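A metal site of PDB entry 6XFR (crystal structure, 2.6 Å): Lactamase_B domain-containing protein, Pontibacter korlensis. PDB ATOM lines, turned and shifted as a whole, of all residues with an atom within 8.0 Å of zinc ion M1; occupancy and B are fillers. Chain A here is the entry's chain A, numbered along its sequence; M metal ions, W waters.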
ATOM      1  N   THR A  77       3.970  -6.889  -6.514  1.00  0.00           N
ATOM      2  CA  THR A  77       5.097  -6.550  -7.393  1.00  0.00           C
ATOM      3  C   THR A  77       5.317  -7.537  -8.542  1.00  0.00           C
ATOM      4  O   THR A  77       6.150  -7.250  -9.420  1.00  0.00           O
ATOM      5  CB  THR A  77       6.411  -6.454  -6.587  1.00  0.00           C
ATOM      6  OG1 THR A  77       6.776  -7.750  -6.058  1.00  0.00           O
ATOM      7  CG2 THR A  77       6.293  -5.419  -5.465  1.00  0.00           C
ATOM      8  N   HIS A  78       4.643  -8.696  -8.528  1.00  0.00           N
ATOM      9  CA  HIS A  78       4.590  -9.617  -9.666  1.00  0.00           C
ATOM     10  C   HIS A  78       3.606 -10.729  -9.306  1.00  0.00           C
ATOM     11  O   HIS A  78       3.018 -10.733  -8.216  1.00  0.00           O
ATOM     12  CB  HIS A  78       5.997 -10.081 -10.059  1.00  0.00           C
ATOM     13  CG  HIS A  78       6.612 -11.092  -9.152  1.00  0.00           C
ATOM     14  ND1 HIS A  78       6.923 -10.824  -7.843  1.00  0.00           N
ATOM     15  CD2 HIS A  78       7.024 -12.360  -9.384  1.00  0.00           C
ATOM     16  CE1 HIS A  78       7.483 -11.888  -7.297  1.00  0.00           C
ATOM     17  NE2 HIS A  78       7.559 -12.829  -8.210  1.00  0.00           N
ATOM     18  N   TRP A  79       3.392 -11.667 -10.244  1.00  0.00           N
ATOM     19  CA  TRP A  79       2.240 -12.572 -10.220  1.00  0.00           C
ATOM     20  C   TRP A  79       2.445 -13.842  -9.371  1.00  0.00           C
ATOM     21  O   TRP A  79       1.495 -14.632  -9.222  1.00  0.00           O
ATOM     22  CB  TRP A  79       1.854 -12.965 -11.652  1.00  0.00           C
ATOM     23  CG  TRP A  79       2.896 -13.799 -12.364  1.00  0.00           C
ATOM     24  CD1 TRP A  79       3.980 -13.334 -13.052  1.00  0.00           C
ATOM     25  CD2 TRP A  79       2.948 -15.224 -12.455  1.00  0.00           C
ATOM     26  NE1 TRP A  79       4.701 -14.381 -13.578  1.00  0.00           N
ATOM     27  CE2 TRP A  79       4.099 -15.556 -13.229  1.00  0.00           C
ATOM     28  CE3 TRP A  79       2.139 -16.271 -11.963  1.00  0.00           C
ATOM     29  CZ2 TRP A  79       4.462 -16.873 -13.527  1.00  0.00           C
ATOM     30  CZ3 TRP A  79       2.495 -17.576 -12.272  1.00  0.00           C
ATOM     31  CH2 TRP A  79       3.663 -17.870 -13.041  1.00  0.00           C
ATOM     32  N   HIS A  80       3.632 -14.063  -8.828  1.00  0.00           N
ATOM     33  CA  HIS A  80       3.867 -15.282  -8.053  1.00  0.00           C
ATOM     34  C   HIS A  80       3.143 -15.234  -6.694  1.00  0.00           C
ATOM     35  O   HIS A  80       2.828 -14.161  -6.162  1.00  0.00           O
ATOM     36  CB  HIS A  80       5.365 -15.532  -7.834  1.00  0.00           C
ATOM     37  CG  HIS A  80       6.096 -16.079  -9.018  1.00  0.00           C
ATOM     38  ND1 HIS A  80       7.480 -16.098  -9.093  1.00  0.00           N
ATOM     39  CD2 HIS A  80       5.653 -16.626 -10.177  1.00  0.00           C
ATOM     40  CE1 HIS A  80       7.854 -16.641 -10.237  1.00  0.00           C
ATOM     41  NE2 HIS A  80       6.766 -16.974 -10.917  1.00  0.00           N
ATOM     42  N   ASP A  81       2.930 -16.425  -6.135  1.00  0.00           N
ATOM     43  CA  ASP A  81       2.133 -16.600  -4.919  1.00  0.00           C
ATOM     44  C   ASP A  81       2.701 -15.842  -3.722  1.00  0.00           C
ATOM     45  O   ASP A  81       1.941 -15.396  -2.859  1.00  0.00           O
ATOM     46  CB  ASP A  81       2.046 -18.099  -4.568  1.00  0.00           C
ATOM     47  CG  ASP A  81       0.729 -18.736  -4.987  1.00  0.00           C
ATOM     48  OD1 ASP A  81      -0.141 -18.069  -5.617  1.00  0.00           O
ATOM     49  OD2 ASP A  81       0.567 -19.939  -4.662  1.00  0.00           O
ATOM     50  N   ASP A  82       4.025 -15.734  -3.605  1.00  0.00           N
ATOM     51  CA  ASP A  82       4.564 -15.053  -2.435  1.00  0.00           C
ATOM     52  C   ASP A  82       4.234 -13.571  -2.418  1.00  0.00           C
ATOM     53  O   ASP A  82       4.092 -12.997  -1.339  1.00  0.00           O
ATOM     54  CB  ASP A  82       6.084 -15.284  -2.317  1.00  0.00           C
ATOM     55  CG  ASP A  82       6.859 -14.855  -3.554  1.00  0.00           C
ATOM     56  OD1 ASP A  82       7.872 -14.124  -3.442  1.00  0.00           O
ATOM     57  OD2 ASP A  82       6.471 -15.267  -4.653  1.00  0.00           O
ATOM     58  N   LYS A  83       3.987 -12.951  -3.557  1.00  0.00           N
ATOM     59  CA  LYS A  83       3.603 -11.543  -3.586  1.00  0.00           C
ATOM     60  C   LYS A  83       2.129 -11.316  -3.897  1.00  0.00           C
ATOM     61  O   LYS A  83       1.633 -10.182  -3.753  1.00  0.00           O
ATOM     62  CB  LYS A  83       4.472 -10.772  -4.616  1.00  0.00           C
ATOM     63  CG  LYS A  83       5.967 -11.205  -4.696  1.00  0.00           C
ATOM     64  CD  LYS A  83       6.892 -10.632  -3.582  1.00  0.00           C
ATOM     65  CE  LYS A  83       6.889 -11.512  -2.331  1.00  0.00           C
ATOM     66  NZ  LYS A  83       7.773 -11.119  -1.173  1.00  0.00           N
ATOM     67  N   HIS A 141      13.587 -11.510 -12.386  1.00  0.00           N
ATOM     68  CA  HIS A 141      13.051 -12.703 -11.708  1.00  0.00           C
ATOM     69  C   HIS A 141      11.807 -13.224 -12.444  1.00  0.00           C
ATOM     70  O   HIS A 141      11.647 -14.431 -12.654  1.00  0.00           O
ATOM     71  CB  HIS A 141      12.775 -12.364 -10.238  1.00  0.00           C
ATOM     72  CG  HIS A 141      11.848 -13.324  -9.564  1.00  0.00           C
ATOM     73  ND1 HIS A 141      12.211 -14.619  -9.268  1.00  0.00           N
ATOM     74  CD2 HIS A 141      10.583 -13.184  -9.115  1.00  0.00           C
ATOM     75  CE1 HIS A 141      11.191 -15.235  -8.706  1.00  0.00           C
ATOM     76  NE2 HIS A 141      10.194 -14.386  -8.593  1.00  0.00           N
ATOM     77  N   THR A 142      10.934 -12.317 -12.860  1.00  0.00           N
ATOM     78  CA  THR A 142       9.812 -12.669 -13.717  1.00  0.00           C
ATOM     79  C   THR A 142       9.719 -11.580 -14.789  1.00  0.00           C
ATOM     80  O   THR A 142      10.339 -10.528 -14.672  1.00  0.00           O
ATOM     81  CB  THR A 142       8.490 -12.772 -12.937  1.00  0.00           C
ATOM     82  OG1 THR A 142       8.361 -11.627 -12.076  1.00  0.00           O
ATOM     83  CG2 THR A 142       8.388 -14.023 -12.091  1.00  0.00           C
ATOM     84  N   ASP A 144       7.409  -9.550 -15.417  1.00  0.00           N
ATOM     85  CA  ASP A 144       6.587  -8.392 -15.092  1.00  0.00           C
ATOM     86  C   ASP A 144       6.983  -7.685 -13.798  1.00  0.00           C
ATOM     87  O   ASP A 144       6.328  -6.704 -13.442  1.00  0.00           O
ATOM     88  CB  ASP A 144       5.112  -8.808 -15.023  1.00  0.00           C
ATOM     89  CG  ASP A 144       4.794  -9.651 -13.799  1.00  0.00           C
ATOM     90  OD1 ASP A 144       4.185  -9.138 -12.823  1.00  0.00           O
ATOM     91  OD2 ASP A 144       5.138 -10.842 -13.795  1.00  0.00           O
ATOM     92  N   ASN A 145       8.055  -8.115 -13.119  1.00  0.00           N
ATOM     93  CA  ASN A 145       8.391  -7.584 -11.793  1.00  0.00           C
ATOM     94  C   ASN A 145       8.596  -6.065 -11.813  1.00  0.00           C
ATOM     95  O   ASN A 145       9.227  -5.509 -12.724  1.00  0.00           O
ATOM     96  CB  ASN A 145       9.637  -8.264 -11.177  1.00  0.00           C
ATOM     97  CG  ASN A 145      10.866  -8.291 -12.103  1.00  0.00           C
ATOM     98  OD1 ASN A 145      11.266  -9.337 -12.578  1.00  0.00           O
ATOM     99  ND2 ASN A 145      11.469  -7.137 -12.332  1.00  0.00           N
ATOM    100  N   GLY A 159      11.657  -6.466  -4.086  1.00  0.00           N
ATOM    101  CA  GLY A 159      11.020  -7.753  -4.270  1.00  0.00           C
ATOM    102  C   GLY A 159      12.002  -8.831  -4.690  1.00  0.00           C
ATOM    103  O   GLY A 159      13.167  -8.836  -4.264  1.00  0.00           O
ATOM    104  N   CYS A 160      11.543  -9.748  -5.551  1.00  0.00           N
ATOM    105  CA  CYS A 160      12.371 -10.883  -5.951  1.00  0.00           C
ATOM    106  C   CYS A 160      13.321 -10.584  -7.095  1.00  0.00           C
ATOM    107  O   CYS A 160      14.098 -11.455  -7.495  1.00  0.00           O
ATOM    108  CB  CYS A 160      11.479 -12.072  -6.302  1.00  0.00           C
ATOM    109  SG  CYS A 160      10.079 -12.238  -5.185  1.00  0.00           S
ATOM    110  N   LEU A 161      13.300  -9.345  -7.591  1.00  0.00           N
ATOM    111  CA  LEU A 161      14.287  -8.890  -8.562  1.00  0.00           C
ATOM    112  C   LEU A 161      15.691  -8.735  -7.960  1.00  0.00           C
ATOM    113  O   LEU A 161      16.698  -8.872  -8.669  1.00  0.00           O
ATOM    114  CB  LEU A 161      13.793  -7.556  -9.099  1.00  0.00           C
ATOM    115  CG  LEU A 161      14.628  -6.814 -10.123  1.00  0.00           C
ATOM    116  CD1 LEU A 161      14.803  -7.680 -11.391  1.00  0.00           C
ATOM    117  CD2 LEU A 161      13.923  -5.522 -10.428  1.00  0.00           C
ATOM    118  N   ASN A 172      14.879 -19.270  -7.456  1.00  0.00           N
ATOM    119  CA  ASN A 172      13.879 -19.697  -8.423  1.00  0.00           C
ATOM    120  C   ASN A 172      14.090 -18.887  -9.697  1.00  0.00           C
ATOM    121  O   ASN A 172      14.123 -17.646  -9.677  1.00  0.00           O
ATOM    122  CB  ASN A 172      12.468 -19.493  -7.881  1.00  0.00           C
ATOM    123  CG  ASN A 172      11.420 -20.244  -8.689  1.00  0.00           C
ATOM    124  OD1 ASN A 172      11.749 -21.155  -9.435  1.00  0.00           O
ATOM    125  ND2 ASN A 172      10.171 -19.830  -8.557  1.00  0.00           N
ATOM    126  N   ASP A 175      10.291 -19.028 -14.161  1.00  0.00           N
ATOM    127  CA  ASP A 175       9.717 -17.934 -14.937  1.00  0.00           C
ATOM    128  C   ASP A 175      10.679 -16.794 -15.180  1.00  0.00           C
ATOM    129  O   ASP A 175      10.239 -15.718 -15.564  1.00  0.00           O
ATOM    130  CB  ASP A 175       8.461 -17.439 -14.241  1.00  0.00           C
ATOM    131  CG  ASP A 175       7.504 -18.579 -13.923  1.00  0.00           C
ATOM    132  OD1 ASP A 175       7.297 -18.832 -12.713  1.00  0.00           O
ATOM    133  OD2 ASP A 175       6.984 -19.233 -14.867  1.00  0.00           O
ATOM    134  N   SER A 201      13.185  -9.816  -1.433  1.00  0.00           N
ATOM    135  CA  SER A 201      12.045 -10.584  -0.978  1.00  0.00           C
ATOM    136  C   SER A 201      12.449 -11.712  -0.046  1.00  0.00           C
ATOM    137  O   SER A 201      11.778 -11.966   0.954  1.00  0.00           O
ATOM    138  CB  SER A 201      11.294 -11.185  -2.189  1.00  0.00           C
ATOM    139  OG  SER A 201      10.309 -10.304  -2.652  1.00  0.00           O
ATOM    140  N   HIS A 202      13.577 -12.366  -0.331  1.00  0.00           N
ATOM    141  CA  HIS A 202      13.805 -13.682   0.222  1.00  0.00           C
ATOM    142  C   HIS A 202      15.086 -13.730   1.031  1.00  0.00           C
ATOM    143  O   HIS A 202      15.693 -14.790   1.200  1.00  0.00           O
ATOM    144  CB  HIS A 202      13.803 -14.738  -0.877  1.00  0.00           C
ATOM    145  CG  HIS A 202      12.500 -14.834  -1.600  1.00  0.00           C
ATOM    146  ND1 HIS A 202      11.306 -15.078  -0.947  1.00  0.00           N
ATOM    147  CD2 HIS A 202      12.194 -14.714  -2.914  1.00  0.00           C
ATOM    148  CE1 HIS A 202      10.328 -15.115  -1.828  1.00  0.00           C
ATOM    149  NE2 HIS A 202      10.837 -14.902  -3.027  1.00  0.00           N
HETATM  150 ZN    ZN M   1       8.463 -14.687  -7.729  1.00  0.00          ZN
HETATM  151 ZN    ZN M   2       9.513 -14.434  -4.721  1.00  0.00          ZN
HETATM  152 ZN    ZN M   3       3.261 -18.978  -8.084  1.00  0.00          ZN
HETATM  153  O   HOH W   1       9.766 -17.178  -6.764  1.00  0.00           O
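A ring nitrogen (NE2) of His 141 is bound to zinc ion M1, at 2.0 Å.
Zinc ion M1 is bound by a ring nitrogen (NE2) of His 78.
Zinc ion M1 is bound by ND1 of His 80, at 2.2 Å.
Zinc ion M1 has three donor atoms within binding distance.
The side-chain amide oxygen (OD1) of Asn 145 sits at hydrogen-bond distance from the backbone NH (N) of His 141 (3.2 Å).
The side-chain hydroxyl of Ser 201 lies within hydrogen-bond range of the backbone NH of Cys 160 (3.2 Å).
NE2 of His 80 sits at hydrogen-bond distance from OD1 of Asp 175 (2.6 Å).
The side-chain carboxylate of Asp 82 sits close to the side-chain amino group of Lys 83 (3.8 Å).
Asp 82 touches zinc ion M1.
Cys 160 touches zinc ion M1.
The nearest printed residue that does not touch zinc ion M1 is Thr 142 (4.4 Å).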
